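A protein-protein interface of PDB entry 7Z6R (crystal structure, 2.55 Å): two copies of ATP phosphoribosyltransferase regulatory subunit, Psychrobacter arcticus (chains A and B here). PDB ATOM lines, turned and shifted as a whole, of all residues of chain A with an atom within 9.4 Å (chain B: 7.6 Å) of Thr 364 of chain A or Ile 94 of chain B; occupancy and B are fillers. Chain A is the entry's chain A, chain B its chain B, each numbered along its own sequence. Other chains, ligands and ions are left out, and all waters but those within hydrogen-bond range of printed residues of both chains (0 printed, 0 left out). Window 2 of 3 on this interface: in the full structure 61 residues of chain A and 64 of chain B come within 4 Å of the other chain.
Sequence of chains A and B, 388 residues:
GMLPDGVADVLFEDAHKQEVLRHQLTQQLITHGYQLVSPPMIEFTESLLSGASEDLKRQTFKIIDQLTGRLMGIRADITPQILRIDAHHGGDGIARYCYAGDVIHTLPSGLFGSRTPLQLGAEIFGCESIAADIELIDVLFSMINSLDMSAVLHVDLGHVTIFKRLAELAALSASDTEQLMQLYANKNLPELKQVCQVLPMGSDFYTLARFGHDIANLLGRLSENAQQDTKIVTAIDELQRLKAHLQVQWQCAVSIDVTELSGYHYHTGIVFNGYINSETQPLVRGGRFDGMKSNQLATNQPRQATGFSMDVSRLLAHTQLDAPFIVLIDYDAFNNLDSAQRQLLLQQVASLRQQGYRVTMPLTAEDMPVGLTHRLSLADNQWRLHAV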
ATOM      1  N   LEU A 328       5.466  36.837   7.817  1.00  0.00           N
ATOM      2  CA  LEU A 328       6.035  35.861   6.852  1.00  0.00           C
ATOM      3  C   LEU A 328       6.196  36.530   5.484  1.00  0.00           C
ATOM      4  O   LEU A 328       5.183  36.956   4.916  1.00  0.00           O
ATOM      5  CB  LEU A 328       5.114  34.636   6.767  1.00  0.00           C
ATOM      6  CG  LEU A 328       5.649  33.436   5.989  1.00  0.00           C
ATOM      7  CD1 LEU A 328       7.052  33.061   6.430  1.00  0.00           C
ATOM      8  CD2 LEU A 328       4.716  32.251   6.150  1.00  0.00           C
ATOM      9  N   ILE A 329       7.428  36.614   4.987  1.00  0.00           N
ATOM     10  CA  ILE A 329       7.713  36.876   3.547  1.00  0.00           C
ATOM     11  C   ILE A 329       7.091  35.730   2.733  1.00  0.00           C
ATOM     12  O   ILE A 329       7.273  34.573   3.130  1.00  0.00           O
ATOM     13  CB  ILE A 329       9.228  36.985   3.292  1.00  0.00           C
ATOM     14  CG1 ILE A 329       9.896  38.139   4.052  1.00  0.00           C
ATOM     15  CG2 ILE A 329       9.499  37.066   1.801  1.00  0.00           C
ATOM     16  CD1 ILE A 329      11.409  37.995   4.149  1.00  0.00           C
ATOM     17  N   ASP A 330       6.389  36.042   1.641  1.00  0.00           N
ATOM     18  CA  ASP A 330       5.817  35.056   0.675  1.00  0.00           C
ATOM     19  C   ASP A 330       6.965  34.290   0.003  1.00  0.00           C
ATOM     20  O   ASP A 330       7.760  34.924  -0.721  1.00  0.00           O
ATOM     21  CB  ASP A 330       4.912  35.728  -0.370  1.00  0.00           C
ATOM     22  CG  ASP A 330       3.463  35.950   0.056  1.00  0.00           C
ATOM     23  OD1 ASP A 330       3.047  35.403   1.100  1.00  0.00           O
ATOM     24  OD2 ASP A 330       2.749  36.678  -0.661  1.00  0.00           O
ATOM     25  N   TYR A 331       7.058  32.983   0.257  1.00  0.00           N
ATOM     26  CA  TYR A 331       8.127  32.093  -0.268  1.00  0.00           C
ATOM     27  C   TYR A 331       8.208  32.230  -1.793  1.00  0.00           C
ATOM     28  O   TYR A 331       9.277  32.621  -2.309  1.00  0.00           O
ATOM     29  CB  TYR A 331       7.895  30.640   0.164  1.00  0.00           C
ATOM     30  CG  TYR A 331       8.897  29.659  -0.389  1.00  0.00           C
ATOM     31  CD1 TYR A 331      10.210  29.635   0.059  1.00  0.00           C
ATOM     32  CD2 TYR A 331       8.539  28.764  -1.382  1.00  0.00           C
ATOM     33  CE1 TYR A 331      11.137  28.745  -0.458  1.00  0.00           C
ATOM     34  CE2 TYR A 331       9.450  27.861  -1.910  1.00  0.00           C
ATOM     35  CZ  TYR A 331      10.755  27.850  -1.446  1.00  0.00           C
ATOM     36  OH  TYR A 331      11.656  26.963  -1.964  1.00  0.00           O
ATOM     37  N   ASP A 332       7.111  31.909  -2.486  1.00  0.00           N
ATOM     38  CA  ASP A 332       7.017  31.857  -3.972  1.00  0.00           C
ATOM     39  C   ASP A 332       7.509  33.175  -4.587  1.00  0.00           C
ATOM     40  O   ASP A 332       8.338  33.140  -5.526  1.00  0.00           O
ATOM     41  CB  ASP A 332       5.580  31.589  -4.427  1.00  0.00           C
ATOM     42  CG  ASP A 332       5.199  30.119  -4.476  1.00  0.00           C
ATOM     43  OD1 ASP A 332       5.485  29.393  -3.502  1.00  0.00           O
ATOM     44  OD2 ASP A 332       4.620  29.711  -5.494  1.00  0.00           O
ATOM     45  N   PHE A 334       9.348  35.680  -3.225  1.00  0.00           N
ATOM     46  CA  PHE A 334      10.774  35.945  -2.895  1.00  0.00           C
ATOM     47  C   PHE A 334      11.694  35.215  -3.882  1.00  0.00           C
ATOM     48  O   PHE A 334      12.701  35.808  -4.300  1.00  0.00           O
ATOM     49  CB  PHE A 334      11.131  35.552  -1.456  1.00  0.00           C
ATOM     50  CG  PHE A 334      12.581  35.824  -1.123  1.00  0.00           C
ATOM     51  CD1 PHE A 334      13.016  37.105  -0.806  1.00  0.00           C
ATOM     52  CD2 PHE A 334      13.529  34.810  -1.189  1.00  0.00           C
ATOM     53  CE1 PHE A 334      14.353  37.362  -0.541  1.00  0.00           C
ATOM     54  CE2 PHE A 334      14.867  35.067  -0.915  1.00  0.00           C
ATOM     55  CZ  PHE A 334      15.276  36.342  -0.587  1.00  0.00           C
ATOM     56  N   ASN A 335      11.371  33.971  -4.241  1.00  0.00           N
ATOM     57  CA  ASN A 335      12.231  33.134  -5.120  1.00  0.00           C
ATOM     58  C   ASN A 335      12.226  33.691  -6.551  1.00  0.00           C
ATOM     59  O   ASN A 335      13.270  33.581  -7.217  1.00  0.00           O
ATOM     60  CB  ASN A 335      11.820  31.664  -5.063  1.00  0.00           C
ATOM     61  CG  ASN A 335      12.341  30.985  -3.820  1.00  0.00           C
ATOM     62  OD1 ASN A 335      11.608  30.794  -2.853  1.00  0.00           O
ATOM     63  ND2 ASN A 335      13.619  30.648  -3.835  1.00  0.00           N
ATOM     64  N   THR A 360      10.278  36.459   9.219  1.00  0.00           N
ATOM     65  CA  THR A 360      10.834  35.145   8.804  1.00  0.00           C
ATOM     66  C   THR A 360      11.042  35.155   7.290  1.00  0.00           C
ATOM     67  O   THR A 360      10.047  35.339   6.571  1.00  0.00           O
ATOM     68  CB  THR A 360       9.896  34.014   9.248  1.00  0.00           C
ATOM     69  OG1 THR A 360       9.696  34.184  10.650  1.00  0.00           O
ATOM     70  CG2 THR A 360      10.428  32.623   8.969  1.00  0.00           C
ATOM     71  N   MET A 361      12.291  34.998   6.844  1.00  0.00           N
ATOM     72  CA  MET A 361      12.629  34.598   5.454  1.00  0.00           C
ATOM     73  C   MET A 361      12.396  33.085   5.373  1.00  0.00           C
ATOM     74  O   MET A 361      13.129  32.306   6.000  1.00  0.00           O
ATOM     75  CB  MET A 361      14.078  34.957   5.096  1.00  0.00           C
ATOM     76  N   PRO A 362      11.331  32.633   4.661  1.00  0.00           N
ATOM     77  CA  PRO A 362      10.919  31.226   4.675  1.00  0.00           C
ATOM     78  C   PRO A 362      11.902  30.324   3.924  1.00  0.00           C
ATOM     79  O   PRO A 362      12.333  30.711   2.859  1.00  0.00           O
ATOM     80  CB  PRO A 362       9.561  31.205   3.961  1.00  0.00           C
ATOM     81  CG  PRO A 362       9.615  32.424   3.057  1.00  0.00           C
ATOM     82  CD  PRO A 362      10.447  33.450   3.810  1.00  0.00           C
ATOM     83  N   LEU A 363      12.225  29.165   4.505  1.00  0.00           N
ATOM     84  CA  LEU A 363      13.133  28.156   3.897  1.00  0.00           C
ATOM     85  C   LEU A 363      12.351  27.323   2.880  1.00  0.00           C
ATOM     86  O   LEU A 363      12.984  26.756   1.979  1.00  0.00           O
ATOM     87  CB  LEU A 363      13.689  27.251   4.995  1.00  0.00           C
ATOM     88  CG  LEU A 363      14.625  27.904   6.001  1.00  0.00           C
ATOM     89  CD1 LEU A 363      14.736  27.029   7.244  1.00  0.00           C
ATOM     90  CD2 LEU A 363      15.986  28.143   5.374  1.00  0.00           C
ATOM     91  N   THR A 364      11.029  27.226   3.059  1.00  0.00           N
ATOM     92  CA  THR A 364      10.103  26.423   2.217  1.00  0.00           C
ATOM     93  C   THR A 364       8.742  27.126   2.138  1.00  0.00           C
ATOM     94  O   THR A 364       8.526  28.087   2.895  1.00  0.00           O
ATOM     95  CB  THR A 364       9.954  24.991   2.766  1.00  0.00           C
ATOM     96  OG1 THR A 364       9.028  24.961   3.854  1.00  0.00           O
ATOM     97  CG2 THR A 364      11.264  24.387   3.220  1.00  0.00           C
ATOM     98  N   ALA A 365       7.851  26.624   1.279  1.00  0.00           N
ATOM     99  CA  ALA A 365       6.445  27.074   1.138  1.00  0.00           C
ATOM    100  C   ALA A 365       5.646  26.791   2.422  1.00  0.00           C
ATOM    101  O   ALA A 365       4.632  27.484   2.639  1.00  0.00           O
ATOM    102  CB  ALA A 365       5.810  26.411  -0.058  1.00  0.00           C
ATOM    103  N   GLU A 366       6.078  25.836   3.254  1.00  0.00           N
ATOM    104  CA  GLU A 366       5.303  25.360   4.433  1.00  0.00           C
ATOM    105  C   GLU A 366       5.792  26.053   5.712  1.00  0.00           C
ATOM    106  O   GLU A 366       5.036  26.057   6.694  1.00  0.00           O
ATOM    107  CB  GLU A 366       5.397  23.838   4.570  1.00  0.00           C
ATOM    108  CG  GLU A 366       4.862  23.075   3.368  1.00  0.00           C
ATOM    109  CD  GLU A 366       5.814  22.995   2.187  1.00  0.00           C
ATOM    110  OE1 GLU A 366       7.037  22.924   2.407  1.00  0.00           O
ATOM    111  OE2 GLU A 366       5.329  23.008   1.044  1.00  0.00           O
ATOM    112  N   ASP A 367       6.999  26.632   5.688  1.00  0.00           N
ATOM    113  CA  ASP A 367       7.625  27.379   6.809  1.00  0.00           C
ATOM    114  C   ASP A 367       6.639  28.456   7.284  1.00  0.00           C
ATOM    115  O   ASP A 367       6.440  29.444   6.556  1.00  0.00           O
ATOM    116  CB  ASP A 367       8.980  27.935   6.364  1.00  0.00           C
ATOM    117  CG  ASP A 367       9.850  28.513   7.470  1.00  0.00           C
ATOM    118  OD1 ASP A 367       9.380  28.587   8.622  1.00  0.00           O
ATOM    119  OD2 ASP A 367      11.009  28.889   7.161  1.00  0.00           O
ATOM    120  N   MET A 368       6.042  28.243   8.462  1.00  0.00           N
ATOM    121  CA  MET A 368       4.971  29.063   9.081  1.00  0.00           C
ATOM    122  C   MET A 368       5.433  29.477  10.476  1.00  0.00           C
ATOM    123  O   MET A 368       5.650  28.624  11.332  1.00  0.00           O
ATOM    124  CB  MET A 368       3.691  28.229   9.214  1.00  0.00           C
ATOM    125  CG  MET A 368       2.427  29.030   9.477  1.00  0.00           C
ATOM    126  SD  MET A 368       1.836  29.987   8.056  1.00  0.00           S
ATOM    127  CE  MET A 368       2.083  28.843   6.696  1.00  0.00           C
ATOM    128  N   PRO A 369       5.611  30.782  10.780  1.00  0.00           N
ATOM    129  CA  PRO A 369       5.938  31.193  12.145  1.00  0.00           C
ATOM    130  C   PRO A 369       4.752  30.985  13.105  1.00  0.00           C
ATOM    131  O   PRO A 369       3.606  31.096  12.677  1.00  0.00           O
ATOM    132  CB  PRO A 369       6.295  32.679  12.016  1.00  0.00           C
ATOM    133  CG  PRO A 369       6.460  32.928  10.524  1.00  0.00           C
ATOM    134  CD  PRO A 369       5.571  31.909   9.842  1.00  0.00           C
ATOM    135  N   VAL A 370       5.046  30.717  14.377  1.00  0.00           N
ATOM    136  CA  VAL A 370       4.035  30.564  15.463  1.00  0.00           C
ATOM    137  C   VAL A 370       3.387  31.930  15.697  1.00  0.00           C
ATOM    138  O   VAL A 370       4.134  32.922  15.825  1.00  0.00           O
ATOM    139  CB  VAL A 370       4.667  30.018  16.761  1.00  0.00           C
ATOM    140  CG1 VAL A 370       3.636  29.854  17.867  1.00  0.00           C
ATOM    141  CG2 VAL A 370       5.424  28.715  16.540  1.00  0.00           C
ATOM    142  N   ARG A 375       1.460  38.756   6.492  1.00  0.00           N
ATOM    143  CA  ARG A 375       2.360  38.317   5.397  1.00  0.00           C
ATOM    144  C   ARG A 375       2.907  39.583   4.744  1.00  0.00           C
ATOM    145  O   ARG A 375       2.182  40.591   4.721  1.00  0.00           O
ATOM    146  CB  ARG A 375       1.625  37.451   4.370  1.00  0.00           C
ATOM    147  CG  ARG A 375       0.865  36.281   4.976  1.00  0.00           C
ATOM    148  CD  ARG A 375       0.163  35.439   3.927  1.00  0.00           C
ATOM    149  NE  ARG A 375       0.006  34.047   4.342  1.00  0.00           N
ATOM    150  CZ  ARG A 375       0.878  33.064   4.101  1.00  0.00           C
ATOM    151  NH1 ARG A 375       1.996  33.296   3.429  1.00  0.00           N
ATOM    152  NH2 ARG A 375       0.624  31.838   4.532  1.00  0.00           N
ATOM    153  N   GLN B  35      12.298  31.961  18.303  1.00  0.00           N
ATOM    154  CA  GLN B  35      11.485  32.027  19.541  1.00  0.00           C
ATOM    155  C   GLN B  35      12.419  31.953  20.742  1.00  0.00           C
ATOM    156  O   GLN B  35      13.208  30.999  20.813  1.00  0.00           O
ATOM    157  CB  GLN B  35      10.502  30.871  19.584  1.00  0.00           C
ATOM    158  CG  GLN B  35       9.624  30.769  18.354  1.00  0.00           C
ATOM    159  CD  GLN B  35       8.816  29.508  18.462  1.00  0.00           C
ATOM    160  OE1 GLN B  35       7.635  29.569  18.773  1.00  0.00           O
ATOM    161  NE2 GLN B  35       9.469  28.374  18.260  1.00  0.00           N
ATOM    162  N   ASP B  86      11.981  21.436  21.952  1.00  0.00           N
ATOM    163  CA  ASP B  86      11.525  21.188  20.549  1.00  0.00           C
ATOM    164  C   ASP B  86      10.725  19.886  20.490  1.00  0.00           C
ATOM    165  O   ASP B  86       9.672  19.895  19.848  1.00  0.00           O
ATOM    166  CB  ASP B  86      12.656  21.138  19.514  1.00  0.00           C
ATOM    167  CG  ASP B  86      12.176  20.733  18.119  1.00  0.00           C
ATOM    168  OD1 ASP B  86      11.500  21.552  17.462  1.00  0.00           O
ATOM    169  OD2 ASP B  86      12.441  19.595  17.706  1.00  0.00           O
ATOM    170  N   GLY B  90       7.687  21.538  19.459  1.00  0.00           N
ATOM    171  CA  GLY B  90       8.208  21.889  18.125  1.00  0.00           C
ATOM    172  C   GLY B  90       7.299  21.510  16.967  1.00  0.00           C
ATOM    173  O   GLY B  90       7.291  22.263  15.972  1.00  0.00           O
ATOM    174  N   GLY B  91       6.592  20.380  17.044  1.00  0.00           N
ATOM    175  CA  GLY B  91       5.865  19.822  15.889  1.00  0.00           C
ATOM    176  C   GLY B  91       6.821  19.125  14.938  1.00  0.00           C
ATOM    177  O   GLY B  91       7.963  18.837  15.337  1.00  0.00           O
ATOM    178  N   ASP B  92       6.359  18.816  13.721  1.00  0.00           N
ATOM    179  CA  ASP B  92       7.114  18.037  12.701  1.00  0.00           C
ATOM    180  C   ASP B  92       7.712  18.984  11.645  1.00  0.00           C
ATOM    181  O   ASP B  92       8.677  18.578  10.977  1.00  0.00           O
ATOM    182  N   GLY B  93       7.167  20.198  11.511  1.00  0.00           N
ATOM    183  CA  GLY B  93       7.640  21.216  10.562  1.00  0.00           C
ATOM    184  C   GLY B  93       8.814  22.002  11.113  1.00  0.00           C
ATOM    185  O   GLY B  93       9.267  21.698  12.220  1.00  0.00           O
ATOM    186  N   ILE B  94       9.280  22.992  10.347  1.00  0.00           N
ATOM    187  CA  ILE B  94      10.397  23.910  10.722  1.00  0.00           C
ATOM    188  C   ILE B  94      10.019  24.629  12.021  1.00  0.00           C
ATOM    189  O   ILE B  94       8.860  25.049  12.149  1.00  0.00           O
ATOM    190  CB  ILE B  94      10.691  24.901   9.578  1.00  0.00           C
ATOM    191  CG1 ILE B  94      11.343  24.194   8.389  1.00  0.00           C
ATOM    192  CG2 ILE B  94      11.527  26.080  10.067  1.00  0.00           C
ATOM    193  CD1 ILE B  94      11.228  24.968   7.098  1.00  0.00           C
ATOM    194  N   ALA B  95      10.975  24.742  12.942  1.00  0.00           N
ATOM    195  CA  ALA B  95      10.868  25.492  14.215  1.00  0.00           C
ATOM    196  C   ALA B  95      12.191  26.209  14.503  1.00  0.00           C
ATOM    197  O   ALA B  95      13.267  25.651  14.176  1.00  0.00           O
ATOM    198  CB  ALA B  95      10.511  24.558  15.338  1.00  0.00           C
ATOM    199  N   ARG B  96      12.104  27.409  15.086  1.00  0.00           N
ATOM    200  CA  ARG B  96      13.280  28.266  15.373  1.00  0.00           C
ATOM    201  C   ARG B  96      13.262  28.650  16.850  1.00  0.00           C
ATOM    202  O   ARG B  96      12.194  29.033  17.368  1.00  0.00           O
ATOM    203  CB  ARG B  96      13.272  29.532  14.511  1.00  0.00           C
ATOM    204  CG  ARG B  96      13.370  29.281  13.014  1.00  0.00           C
ATOM    205  CD  ARG B  96      13.472  30.594  12.279  1.00  0.00           C
ATOM    206  NE  ARG B  96      13.662  30.457  10.850  1.00  0.00           N
ATOM    207  CZ  ARG B  96      12.728  30.073   9.996  1.00  0.00           C
ATOM    208  NH1 ARG B  96      11.519  29.757  10.430  1.00  0.00           N
ATOM    209  NH2 ARG B  96      13.016  29.999   8.707  1.00  0.00           N
ATOM    210  N   TYR B  97      14.415  28.551  17.497  1.00  0.00           N
ATOM    211  CA  TYR B  97      14.586  28.891  18.917  1.00  0.00           C
ATOM    212  C   TYR B  97      15.872  29.698  19.036  1.00  0.00           C
ATOM    213  O   TYR B  97      16.830  29.396  18.301  1.00  0.00           O
ATOM    214  CB  TYR B  97      14.606  27.628  19.792  1.00  0.00           C
ATOM    215  CG  TYR B  97      13.495  26.646  19.525  1.00  0.00           C
ATOM    216  CD1 TYR B  97      12.240  26.790  20.092  1.00  0.00           C
ATOM    217  CD2 TYR B  97      13.709  25.570  18.681  1.00  0.00           C
ATOM    218  CE1 TYR B  97      11.216  25.898  19.826  1.00  0.00           C
ATOM    219  CE2 TYR B  97      12.702  24.660  18.413  1.00  0.00           C
ATOM    220  CZ  TYR B  97      11.454  24.817  18.994  1.00  0.00           C
ATOM    221  OH  TYR B  97      10.488  23.889  18.729  1.00  0.00           O
ATOM    222  N   ILE B 124      17.784  26.003  14.252  1.00  0.00           N
ATOM    223  CA  ILE B 124      16.691  25.657  13.291  1.00  0.00           C
ATOM    224  C   ILE B 124      16.516  24.136  13.267  1.00  0.00           C
ATOM    225  O   ILE B 124      17.481  23.425  12.884  1.00  0.00           O
ATOM    226  CB  ILE B 124      16.973  26.210  11.879  1.00  0.00           C
ATOM    227  CG1 ILE B 124      17.324  27.703  11.947  1.00  0.00           C
ATOM    228  CG2 ILE B 124      15.787  25.929  10.968  1.00  0.00           C
ATOM    229  CD1 ILE B 124      17.673  28.343  10.625  1.00  0.00           C
ATOM    230  N   PHE B 125      15.311  23.689  13.627  1.00  0.00           N
ATOM    231  CA  PHE B 125      14.857  22.278  13.558  1.00  0.00           C
ATOM    232  C   PHE B 125      13.927  22.091  12.352  1.00  0.00           C
ATOM    233  O   PHE B 125      13.107  23.007  12.108  1.00  0.00           O
ATOM    234  CB  PHE B 125      14.158  21.907  14.866  1.00  0.00           C
ATOM    235  CG  PHE B 125      15.066  21.828  16.069  1.00  0.00           C
ATOM    236  CD1 PHE B 125      15.557  22.981  16.650  1.00  0.00           C
ATOM    237  CD2 PHE B 125      15.435  20.606  16.619  1.00  0.00           C
ATOM    238  CE1 PHE B 125      16.384  22.920  17.764  1.00  0.00           C
ATOM    239  CE2 PHE B 125      16.283  20.547  17.712  1.00  0.00           C
ATOM    240  CZ  PHE B 125      16.762  21.706  18.281  1.00  0.00           C
ATOM    241  N   GLY B 126      14.076  20.969  11.620  1.00  0.00           N
ATOM    242  CA  GLY B 126      13.066  20.439  10.680  1.00  0.00           C
ATOM    243  C   GLY B 126      13.310  20.782   9.216  1.00  0.00           C
ATOM    244  O   GLY B 126      12.350  20.620   8.423  1.00  0.00           O
ATOM    245  N   CYS B 127      14.523  21.216   8.838  1.00  0.00           N
ATOM    246  CA  CYS B 127      14.911  21.566   7.440  1.00  0.00           C
ATOM    247  C   CYS B 127      16.189  20.817   7.036  1.00  0.00           C
ATOM    248  O   CYS B 127      17.215  20.981   7.709  1.00  0.00           O
ATOM    249  CB  CYS B 127      15.124  23.071   7.281  1.00  0.00           C
ATOM    250  SG  CYS B 127      15.557  23.594   5.593  1.00  0.00           S
ATOM    251  N   GLU B 128      16.111  20.017   5.972  1.00  0.00           N
ATOM    252  CA  GLU B 128      17.259  19.257   5.407  1.00  0.00           C
ATOM    253  C   GLU B 128      18.172  20.234   4.655  1.00  0.00           C
ATOM    254  O   GLU B 128      19.401  20.118   4.791  1.00  0.00           O
ATOM    255  N   SER B 129      17.571  21.159   3.893  1.00  0.00           N
ATOM    256  CA  SER B 129      18.253  22.117   2.983  1.00  0.00           C
ATOM    257  C   SER B 129      19.397  22.802   3.726  1.00  0.00           C
ATOM    258  O   SER B 129      19.187  23.211   4.876  1.00  0.00           O
ATOM    259  CB  SER B 129      17.293  23.149   2.432  1.00  0.00           C
ATOM    260  OG  SER B 129      17.933  23.990   1.470  1.00  0.00           O
ATOM    261  N   ALA B 131      20.021  25.600   3.058  1.00  0.00           N
ATOM    262  CA  ALA B 131      19.356  26.921   3.139  1.00  0.00           C
ATOM    263  C   ALA B 131      19.263  27.374   4.608  1.00  0.00           C
ATOM    264  O   ALA B 131      19.512  28.569   4.880  1.00  0.00           O
ATOM    265  CB  ALA B 131      17.998  26.863   2.489  1.00  0.00           C
ATOM    266  N   ALA B 132      18.926  26.457   5.518  1.00  0.00           N
ATOM    267  CA  ALA B 132      18.820  26.720   6.973  1.00  0.00           C
ATOM    268  C   ALA B 132      20.196  27.072   7.540  1.00  0.00           C
ATOM    269  O   ALA B 132      20.241  27.957   8.400  1.00  0.00           O
ATOM    270  CB  ALA B 132      18.209  25.540   7.703  1.00  0.00           C
ATOM    271  N   GLU B 135      20.877  30.559   6.563  1.00  0.00           N
ATOM    272  CA  GLU B 135      20.017  31.473   7.362  1.00  0.00           C
ATOM    273  C   GLU B 135      20.700  31.764   8.707  1.00  0.00           C
ATOM    274  O   GLU B 135      20.752  32.950   9.093  1.00  0.00           O
ATOM    275  CB  GLU B 135      18.615  30.899   7.570  1.00  0.00           C
ATOM    276  CG  GLU B 135      17.676  31.904   8.217  1.00  0.00           C
ATOM    277  CD  GLU B 135      16.269  31.418   8.494  1.00  0.00           C
ATOM    278  OE1 GLU B 135      15.620  30.905   7.553  1.00  0.00           O
ATOM    279  OE2 GLU B 135      15.822  31.573   9.648  1.00  0.00           O
ATOM    280  N   ARG B 303      14.786  13.982  13.320  1.00  0.00           N
ATOM    281  CA  ARG B 303      14.577  15.462  13.313  1.00  0.00           C
ATOM    282  C   ARG B 303      15.877  16.184  12.938  1.00  0.00           C
ATOM    283  O   ARG B 303      16.828  16.193  13.743  1.00  0.00           O
ATOM    284  CB  ARG B 303      14.047  15.934  14.672  1.00  0.00           C
ATOM    285  CG  ARG B 303      13.749  17.422  14.748  1.00  0.00           C
ATOM    286  CD  ARG B 303      12.267  17.686  14.806  1.00  0.00           C
ATOM    287  NE  ARG B 303      12.041  19.119  14.745  1.00  0.00           N
ATOM    288  CZ  ARG B 303      10.967  19.698  14.233  1.00  0.00           C
ATOM    289  NH1 ARG B 303      10.001  18.970  13.705  1.00  0.00           N
ATOM    290  NH2 ARG B 303      10.845  21.009  14.234  1.00  0.00           N
ATOM    291  N   GLN B 304      15.893  16.793  11.757  1.00  0.00           N
ATOM    292  CA  GLN B 304      17.046  17.568  11.227  1.00  0.00           C
ATOM    293  C   GLN B 304      17.159  18.868  12.044  1.00  0.00           C
ATOM    294  O   GLN B 304      16.113  19.404  12.510  1.00  0.00           O
ATOM    295  CB  GLN B 304      16.897  17.727   9.704  1.00  0.00           C
ATOM    296  CG  GLN B 304      15.557  18.305   9.222  1.00  0.00           C
ATOM    297  CD  GLN B 304      14.328  17.411   9.152  1.00  0.00           C
ATOM    298  OE1 GLN B 304      13.811  16.920  10.165  1.00  0.00           O
ATOM    299  NE2 GLN B 304      13.769  17.288   7.954  1.00  0.00           N
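OD2 of Asp 367 of chain A is in salt-bridge range of NH2 of Arg 96 of chain B, at 2.8 Å. The side-chain carboxylate of Glu 135 of chain B lies close to the backbone carbonyl oxygen of Met 361 of chain A, at 3.3 Å.
The side-chain carboxylate (OE2) of Glu 135 of chain B is in salt-bridge range of the guanidinium group (NE) of Arg 96 of chain B, at 2.7 Å. The backbone NH (N) of Ile 329 of chain A sits at hydrogen-bond distance from the backbone carbonyl oxygen (O) of Thr 360 of chain A, 3.3 Å away. The backbone NH (N) of Leu 363 of chain A lies within hydrogen-bond range of the side-chain carboxylate (OD2) of Asp 367 of chain A (2.9 Å). N of Ala 131 of chain B sits close to OG of Ser 129 of chain B.
CG2 of Thr 360 of chain A touches NH1 of Arg 96 of chain B, 3.4 Å away. Met 361 of chain A touches Arg 96 of chain B. Leu 363 of chain A touches Ile 94 of chain B (CB to CD1, 3.96 Å). Leu 363 of chain A touches Arg 96 of chain B (CD1 to NH2, 3.7 Å). Cys 127 of chain B touches Leu 363 of chain A (SG to CD1, 3.9 Å). Ala 132 of chain B touches Leu 363 of chain A (N to CD2, 3.4 Å). Glu 135 of chain B touches Leu 363 of chain A (OE1 to CG, 3.5 Å). Thr 364 of chain A touches Ile 94 of chain B (OG1 to CD1, 3.9 Å). Asp 367 of chain A touches Ile 94 of chain B (OD1 to CG2, 3.6 Å). Val 370 of chain A touches Gln 35 of chain B (CG2 to OE1, 3.3 Å).
Thr 364 of chain A touches just one residue of chain B: Ile 94 (3.9 Å). Printed residues of chain A within 4 Å of Ile 94 of chain B: Leu 363 (3.96 Å), Thr 364 (3.9 Å) and Asp 367 (3.6 Å). No residue of chain A comes within 4 Å of Ala 95 of chain B. No residue of chain A comes within 4 Å of Gly 126 of chain B. Of the printed residues of chain B, Leu 363 of chain A touches Ile 94, Arg 96, Cys 127, Ala 131, Ala 132 and Glu 135. Of the printed residues of chain A, Ala 132 of chain B touches Leu 363. Of the printed residues of chain B, Val 370 of chain A touches Gln 35 (3.3 Å). Of the printed residues of chain B, Met 361 of chain A touches Arg 96 and Glu 135. Asp 86 of chain B touches none of the printed residues of chain A. The nearest residue of chain A that does not touch Ile 94 of chain B is Met 368 of chain A (4.9 Å). The nearest printed residue of chain A that does not touch Ala 131 of chain B is Pro 362 of chain A (6.9 Å).
Printed residues of chain B that touch a printed residue of chain A: Gln 35, Ile 94, Arg 96, Cys 127, Ala 131, Ala 132 and Glu 135. Hydrophobic or aromatic side chains of chain B that line the printed part of chain A: Ile 94, Ala 131 and Ala 132. Printed residues of chain A that touch a printed residue of chain B: Thr 360, Met 361, Leu 363, Thr 364, Asp 367 and Val 370. Among the printed residues, 13 pairs touch across the chains. Among the printed residues, Asp or Glu carboxylates within 4 Å of a Lys or Arg side-chain nitrogen of the other chain: Asp 367 of chain A with Arg 96 of chain B.
No position is printed for both chains.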
